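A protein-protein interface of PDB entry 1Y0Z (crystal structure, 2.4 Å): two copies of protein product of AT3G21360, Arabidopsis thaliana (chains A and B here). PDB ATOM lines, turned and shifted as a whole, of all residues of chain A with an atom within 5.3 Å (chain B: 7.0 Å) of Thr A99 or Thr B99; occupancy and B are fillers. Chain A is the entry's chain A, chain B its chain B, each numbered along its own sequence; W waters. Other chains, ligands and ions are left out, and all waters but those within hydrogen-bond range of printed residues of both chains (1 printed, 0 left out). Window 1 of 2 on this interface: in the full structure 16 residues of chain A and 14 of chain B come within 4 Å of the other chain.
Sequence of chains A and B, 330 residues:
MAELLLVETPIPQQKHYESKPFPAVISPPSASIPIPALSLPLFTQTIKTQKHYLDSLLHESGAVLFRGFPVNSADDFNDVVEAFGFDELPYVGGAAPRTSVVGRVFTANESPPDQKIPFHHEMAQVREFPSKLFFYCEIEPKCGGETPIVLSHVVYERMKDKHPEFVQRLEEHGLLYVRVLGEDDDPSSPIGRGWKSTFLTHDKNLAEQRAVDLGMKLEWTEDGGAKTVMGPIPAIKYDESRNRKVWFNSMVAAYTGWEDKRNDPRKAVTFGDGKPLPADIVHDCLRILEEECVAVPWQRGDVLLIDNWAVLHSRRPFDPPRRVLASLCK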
ATOM      1  N   PRO A  97      18.730  -4.188  16.613  1.00  0.00           N
ATOM      2  CA  PRO A  97      18.867  -4.398  18.070  1.00  0.00           C
ATOM      3  C   PRO A  97      20.276  -4.768  18.512  1.00  0.00           C
ATOM      4  O   PRO A  97      20.657  -5.943  18.530  1.00  0.00           O
ATOM      5  CB  PRO A  97      17.857  -5.514  18.393  1.00  0.00           C
ATOM      6  CG  PRO A  97      17.280  -5.944  17.074  1.00  0.00           C
ATOM      7  CD  PRO A  97      17.469  -4.775  16.132  1.00  0.00           C
ATOM      8  N   ARG A  98      21.033  -3.740  18.883  1.00  0.00           N
ATOM      9  CA  ARG A  98      22.412  -3.893  19.320  1.00  0.00           C
ATOM     10  C   ARG A  98      22.604  -4.151  20.814  1.00  0.00           C
ATOM     11  O   ARG A  98      21.864  -3.633  21.656  1.00  0.00           O
ATOM     12  CB  ARG A  98      23.217  -2.660  18.915  1.00  0.00           C
ATOM     13  CG  ARG A  98      24.162  -2.941  17.768  1.00  0.00           C
ATOM     14  CD  ARG A  98      24.436  -1.705  16.928  1.00  0.00           C
ATOM     15  NE  ARG A  98      25.439  -0.812  17.504  1.00  0.00           N
ATOM     16  CZ  ARG A  98      25.920   0.258  16.879  1.00  0.00           C
ATOM     17  NH1 ARG A  98      25.487   0.564  15.662  1.00  0.00           N
ATOM     18  NH2 ARG A  98      26.840   1.020  17.461  1.00  0.00           N
ATOM     19  N   THR A  99      23.614  -4.953  21.140  1.00  0.00           N
ATOM     20  CA  THR A  99      23.913  -5.260  22.531  1.00  0.00           C
ATOM     21  C   THR A  99      25.399  -5.054  22.821  1.00  0.00           C
ATOM     22  O   THR A  99      26.251  -5.819  22.367  1.00  0.00           O
ATOM     23  CB  THR A  99      23.521  -6.706  22.880  1.00  0.00           C
ATOM     24  OG1 THR A  99      22.164  -6.936  22.490  1.00  0.00           O
ATOM     25  CG2 THR A  99      23.634  -6.939  24.373  1.00  0.00           C
ATOM     26  N   SER A 100      25.696  -4.007  23.580  1.00  0.00           N
ATOM     27  CA  SER A 100      27.064  -3.667  23.952  1.00  0.00           C
ATOM     28  C   SER A 100      27.659  -4.735  24.872  1.00  0.00           C
ATOM     29  O   SER A 100      27.017  -5.164  25.830  1.00  0.00           O
ATOM     30  CB  SER A 100      27.072  -2.306  24.650  1.00  0.00           C
ATOM     31  OG  SER A 100      28.387  -1.910  24.980  1.00  0.00           O
ATOM     32  N   VAL A 101      28.877  -5.168  24.568  1.00  0.00           N
ATOM     33  CA  VAL A 101      29.553  -6.187  25.366  1.00  0.00           C
ATOM     34  C   VAL A 101      30.529  -5.484  26.310  1.00  0.00           C
ATOM     35  O   VAL A 101      30.422  -5.590  27.529  1.00  0.00           O
ATOM     36  CB  VAL A 101      30.339  -7.156  24.463  1.00  0.00           C
ATOM     37  CG1 VAL A 101      30.887  -8.318  25.281  1.00  0.00           C
ATOM     38  CG2 VAL A 101      29.450  -7.633  23.329  1.00  0.00           C
ATOM     39  N   VAL A 105      32.866  -2.510  21.697  1.00  0.00           N
ATOM     40  CA  VAL A 105      32.503  -3.800  21.124  1.00  0.00           C
ATOM     41  C   VAL A 105      31.063  -4.194  21.401  1.00  0.00           C
ATOM     42  O   VAL A 105      30.550  -3.985  22.497  1.00  0.00           O
ATOM     43  CB  VAL A 105      33.433  -4.902  21.651  1.00  0.00           C
ATOM     44  CG1 VAL A 105      33.053  -6.235  21.031  1.00  0.00           C
ATOM     45  CG2 VAL A 105      34.893  -4.537  21.333  1.00  0.00           C
ATOM     46  N   PHE A 106      30.408  -4.768  20.402  1.00  0.00           N
ATOM     47  CA  PHE A 106      29.027  -5.182  20.579  1.00  0.00           C
ATOM     48  C   PHE A 106      28.641  -6.410  19.774  1.00  0.00           C
ATOM     49  O   PHE A 106      29.361  -6.830  18.863  1.00  0.00           O
ATOM     50  CB  PHE A 106      28.080  -4.043  20.192  1.00  0.00           C
ATOM     51  CG  PHE A 106      28.125  -3.679  18.726  1.00  0.00           C
ATOM     52  CD1 PHE A 106      29.068  -2.773  18.243  1.00  0.00           C
ATOM     53  CD2 PHE A 106      27.219  -4.242  17.829  1.00  0.00           C
ATOM     54  CE1 PHE A 106      29.108  -2.428  16.888  1.00  0.00           C
ATOM     55  CE2 PHE A 106      27.250  -3.905  16.473  1.00  0.00           C
ATOM     56  CZ  PHE A 106      28.198  -2.994  16.003  1.00  0.00           C
ATOM     57  N   THR A 107      27.488  -6.971  20.132  1.00  0.00           N
ATOM     58  CA  THR A 107      26.926  -8.117  19.442  1.00  0.00           C
ATOM     59  C   THR A 107      25.568  -7.703  18.930  1.00  0.00           C
ATOM     60  O   THR A 107      24.730  -7.186  19.673  1.00  0.00           O
ATOM     61  CB  THR A 107      26.707  -9.339  20.348  1.00  0.00           C
ATOM     62  OG1 THR A 107      26.061  -8.940  21.558  1.00  0.00           O
ATOM     63  CG2 THR A 107      27.998  -9.997  20.666  1.00  0.00           C
ATOM     64  N   ALA A 108      25.361  -7.916  17.644  1.00  0.00           N
ATOM     65  CA  ALA A 108      24.092  -7.589  17.040  1.00  0.00           C
ATOM     66  C   ALA A 108      23.474  -8.916  16.663  1.00  0.00           C
ATOM     67  O   ALA A 108      24.175  -9.856  16.272  1.00  0.00           O
ATOM     68  CB  ALA A 108      24.298  -6.729  15.810  1.00  0.00           C
ATOM     69  N   ASN A 109      22.161  -9.003  16.808  1.00  0.00           N
ATOM     70  CA  ASN A 109      21.465 -10.223  16.471  1.00  0.00           C
ATOM     71  C   ASN A 109      21.033 -10.150  15.019  1.00  0.00           C
ATOM     72  O   ASN A 109      20.227  -9.307  14.613  1.00  0.00           O
ATOM     73  CB  ASN A 109      20.273 -10.423  17.404  1.00  0.00           C
ATOM     74  CG  ASN A 109      19.729  -9.120  17.925  1.00  0.00           C
ATOM     75  OD1 ASN A 109      19.309  -8.261  17.153  1.00  0.00           O
ATOM     76  ND2 ASN A 109      19.739  -8.959  19.243  1.00  0.00           N
ATOM     77  N   ARG A 323      30.318 -17.000  17.131  1.00  0.00           N
ATOM     78  CA  ARG A 323      30.251 -15.708  17.781  1.00  0.00           C
ATOM     79  C   ARG A 323      31.265 -14.772  17.159  1.00  0.00           C
ATOM     80  O   ARG A 323      32.472 -15.002  17.231  1.00  0.00           O
ATOM     81  CB  ARG A 323      30.508 -15.818  19.287  1.00  0.00           C
ATOM     82  CG  ARG A 323      30.052 -14.563  20.016  1.00  0.00           C
ATOM     83  CD  ARG A 323      30.539 -14.470  21.452  1.00  0.00           C
ATOM     84  NE  ARG A 323      29.968 -13.297  22.115  1.00  0.00           N
ATOM     85  CZ  ARG A 323      30.374 -12.810  23.286  1.00  0.00           C
ATOM     86  NH1 ARG A 323      31.368 -13.383  23.950  1.00  0.00           N
ATOM     87  NH2 ARG A 323      29.773 -11.748  23.803  1.00  0.00           N
ATOM     88  N   THR B  99      25.798 -10.675  27.890  1.00  0.00           N
ATOM     89  CA  THR B  99      26.874 -10.800  26.868  1.00  0.00           C
ATOM     90  C   THR B  99      28.246 -11.000  27.499  1.00  0.00           C
ATOM     91  O   THR B  99      28.791 -10.106  28.144  1.00  0.00           O
ATOM     92  CB  THR B  99      26.945  -9.561  25.989  1.00  0.00           C
ATOM     93  OG1 THR B  99      25.645  -9.269  25.468  1.00  0.00           O
ATOM     94  CG2 THR B  99      27.893  -9.805  24.842  1.00  0.00           C
ATOM     95  N   SER B 100      28.804 -12.181  27.275  1.00  0.00           N
ATOM     96  CA  SER B 100      30.102 -12.557  27.814  1.00  0.00           C
ATOM     97  C   SER B 100      31.239 -11.577  27.525  1.00  0.00           C
ATOM     98  O   SER B 100      31.611 -11.357  26.374  1.00  0.00           O
ATOM     99  CB  SER B 100      30.483 -13.939  27.295  1.00  0.00           C
ATOM    100  OG  SER B 100      31.701 -14.350  27.869  1.00  0.00           O
ATOM    101  N   VAL B 101      31.805 -11.004  28.581  1.00  0.00           N
ATOM    102  CA  VAL B 101      32.900 -10.052  28.437  1.00  0.00           C
ATOM    103  C   VAL B 101      34.251 -10.767  28.440  1.00  0.00           C
ATOM    104  O   VAL B 101      35.094 -10.516  27.575  1.00  0.00           O
ATOM    105  CB  VAL B 101      32.863  -8.994  29.566  1.00  0.00           C
ATOM    106  CG1 VAL B 101      34.071  -8.059  29.467  1.00  0.00           C
ATOM    107  CG2 VAL B 101      31.577  -8.193  29.457  1.00  0.00           C
ATOM    108  N   VAL B 102      34.443 -11.652  29.417  1.00  0.00           N
ATOM    109  CA  VAL B 102      35.662 -12.444  29.541  1.00  0.00           C
ATOM    110  C   VAL B 102      35.440 -13.581  30.532  1.00  0.00           C
ATOM    111  O   VAL B 102      34.844 -13.390  31.588  1.00  0.00           O
ATOM    112  CB  VAL B 102      36.880 -11.578  29.990  1.00  0.00           C
ATOM    113  CG1 VAL B 102      36.598 -10.884  31.307  1.00  0.00           C
ATOM    114  CG2 VAL B 102      38.122 -12.450  30.109  1.00  0.00           C
ATOM    115  N   VAL B 105      32.628 -13.990  33.271  1.00  0.00           N
ATOM    116  CA  VAL B 105      32.025 -12.689  33.519  1.00  0.00           C
ATOM    117  C   VAL B 105      31.211 -12.156  32.348  1.00  0.00           C
ATOM    118  O   VAL B 105      31.616 -12.287  31.193  1.00  0.00           O
ATOM    119  CB  VAL B 105      33.108 -11.675  33.884  1.00  0.00           C
ATOM    120  CG1 VAL B 105      32.501 -10.291  34.055  1.00  0.00           C
ATOM    121  CG2 VAL B 105      33.810 -12.131  35.153  1.00  0.00           C
ATOM    122  N   PHE B 106      30.065 -11.554  32.655  1.00  0.00           N
ATOM    123  CA  PHE B 106      29.194 -10.989  31.629  1.00  0.00           C
ATOM    124  C   PHE B 106      28.471  -9.713  32.082  1.00  0.00           C
ATOM    125  O   PHE B 106      28.507  -9.341  33.257  1.00  0.00           O
ATOM    126  CB  PHE B 106      28.148 -12.021  31.194  1.00  0.00           C
ATOM    127  CG  PHE B 106      27.174 -12.402  32.279  1.00  0.00           C
ATOM    128  CD1 PHE B 106      27.519 -13.335  33.255  1.00  0.00           C
ATOM    129  CD2 PHE B 106      25.903 -11.834  32.322  1.00  0.00           C
ATOM    130  CE1 PHE B 106      26.614 -13.699  34.251  1.00  0.00           C
ATOM    131  CE2 PHE B 106      24.985 -12.193  33.319  1.00  0.00           C
ATOM    132  CZ  PHE B 106      25.346 -13.130  34.285  1.00  0.00           C
ATOM    133  N   THR B 107      27.825  -9.048  31.128  1.00  0.00           N
ATOM    134  CA  THR B 107      27.056  -7.838  31.392  1.00  0.00           C
ATOM    135  C   THR B 107      25.590  -8.239  31.260  1.00  0.00           C
ATOM    136  O   THR B 107      25.222  -8.944  30.316  1.00  0.00           O
ATOM    137  CB  THR B 107      27.353  -6.741  30.353  1.00  0.00           C
ATOM    138  OG1 THR B 107      28.759  -6.481  30.329  1.00  0.00           O
ATOM    139  CG2 THR B 107      26.615  -5.454  30.703  1.00  0.00           C
ATOM    140  N   ALA B 108      24.754  -7.799  32.196  1.00  0.00           N
ATOM    141  CA  ALA B 108      23.332  -8.143  32.162  1.00  0.00           C
ATOM    142  C   ALA B 108      22.471  -7.061  31.524  1.00  0.00           C
ATOM    143  O   ALA B 108      22.474  -5.920  31.991  1.00  0.00           O
ATOM    144  CB  ALA B 108      22.844  -8.419  33.573  1.00  0.00           C
ATOM    145  N   ASN B 109      21.730  -7.417  30.471  1.00  0.00           N
ATOM    146  CA  ASN B 109      20.868  -6.439  29.807  1.00  0.00           C
ATOM    147  C   ASN B 109      19.746  -6.028  30.762  1.00  0.00           C
ATOM    148  O   ASN B 109      18.663  -6.611  30.772  1.00  0.00           O
ATOM    149  CB  ASN B 109      20.280  -6.992  28.491  1.00  0.00           C
ATOM    150  CG  ASN B 109      19.470  -8.254  28.680  1.00  0.00           C
ATOM    151  OD1 ASN B 109      19.131  -8.648  29.793  1.00  0.00           O
ATOM    152  ND2 ASN B 109      19.154  -8.902  27.569  1.00  0.00           N
ATOM    153  N   ARG B 323      28.429   0.687  35.419  1.00  0.00           N
ATOM    154  CA  ARG B 323      28.774  -0.587  34.844  1.00  0.00           C
ATOM    155  C   ARG B 323      29.038  -1.612  35.927  1.00  0.00           C
ATOM    156  O   ARG B 323      29.995  -1.494  36.687  1.00  0.00           O
ATOM    157  CB  ARG B 323      29.999  -0.465  33.938  1.00  0.00           C
ATOM    158  CG  ARG B 323      30.180  -1.701  33.100  1.00  0.00           C
ATOM    159  CD  ARG B 323      31.277  -1.616  32.073  1.00  0.00           C
ATOM    160  NE  ARG B 323      31.016  -2.621  31.045  1.00  0.00           N
ATOM    161  CZ  ARG B 323      31.911  -3.484  30.593  1.00  0.00           C
ATOM    162  NH1 ARG B 323      33.144  -3.468  31.076  1.00  0.00           N
ATOM    163  NH2 ARG B 323      31.570  -4.369  29.671  1.00  0.00           N
ATOM    164  N   LEU B 325      29.330  -5.773  36.289  1.00  0.00           N
ATOM    165  CA  LEU B 325      29.399  -7.065  35.621  1.00  0.00           C
ATOM    166  C   LEU B 325      28.918  -8.143  36.596  1.00  0.00           C
ATOM    167  O   LEU B 325      28.793  -7.889  37.797  1.00  0.00           O
ATOM    168  CB  LEU B 325      30.835  -7.346  35.175  1.00  0.00           C
ATOM    169  CG  LEU B 325      31.513  -6.268  34.311  1.00  0.00           C
ATOM    170  CD1 LEU B 325      32.935  -6.700  33.971  1.00  0.00           C
ATOM    171  CD2 LEU B 325      30.717  -6.033  33.037  1.00  0.00           C
HETATM  172  O   HOH W   1      34.389 -12.684  25.464  1.00  0.00           O
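Among the printed residues, merely in contact across the chains: Thr A99 with Thr B99 (3.3 Å), Val A101 with Thr B99 (3.1 Å), Val A101 with Ser B100 (3.3 Å), Val A101 with Val B101 (3.4 Å), Thr A107 with Thr B99 (3.9 Å) and Arg A323 with Thr B99 (2.9 Å).
Of the 11 printed residues of chain B, 5 touch a printed residue of chain A.
Printed residues of chain B that touch a printed residue of chain A: Thr B99, Ser B100, Val B101, Thr B107 and Arg B323.
Hydrophobic or aromatic side chains of chain A within 4 Å of the printed part of chain B: Val A101.
Among the printed residues, no Asp or Glu carboxylate lies within 4 Å of a Lys or Arg side-chain nitrogen of the other chain.
O of Thr A99 lies within hydrogen-bond range of N of Thr A107 (2.8 Å).
The backbone carbonyl oxygen (O) of Thr B107 lies within hydrogen-bond range of the backbone NH (N) of Thr B99 (3.0 Å).
Water W1 lies within hydrogen-bond range of O of Val B101 (3.1 Å), O of Ser B100 (3.2 Å) and NH1 of Arg A323 (3.5 Å).
Of the printed residues of chain B, Val A101 touches Thr B99, Ser B100, Val B101, Thr B107 and Arg B323.
Of the printed residues of chain B, Thr A107 touches Thr B99 (3.9 Å).
Ala A108 touches none of the printed residues of chain B.
Of the printed residues of chain B, Arg A323 touches Thr B99 and Ser B100.
Of chain A, only Thr A99, Val A101, Thr A107 and Arg A323 come within 4 Å of Thr B99.
Of the printed residues of chain A, Val B101 touches Val A101 (3.4 Å).
Of the printed residues of chain A, Thr B107 touches Val A101 (3.4 Å).
Ala B108 touches none of the printed residues of chain A.
The nearest residue of chain B that does not touch Thr A99 is Asn B109 (5.3 Å).
Val A101 touches Thr B99, but with the chains exchanged Thr A99 does not touch Val B101 (9.2 Å).
Val A101 touches Ser B100, but with the chains exchanged Ser A100 does not touch Val B101 (6.6 Å).
Val A101 touches Arg B323, but with the chains exchanged Arg A323 does not touch Val B101 (5.2 Å).
Arg A323 touches Thr B99, but with the chains exchanged Thr A99 does not touch Arg B323 (9.2 Å).
Of the 9 pairs that touch across the chains among the printed residues, 2 have their exchanged pair printed and touching as well.
OG1 of Thr B107 lies within hydrogen-bond range of O of Val A101 (3.4 Å).
The guanidinium group of Arg B323 lies within hydrogen-bond range of the backbone carbonyl oxygen of Val A101 (2.7 Å).
O of Ser B100 sits at hydrogen-bond distance from NH1 of Arg A323, at 3.2 Å.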
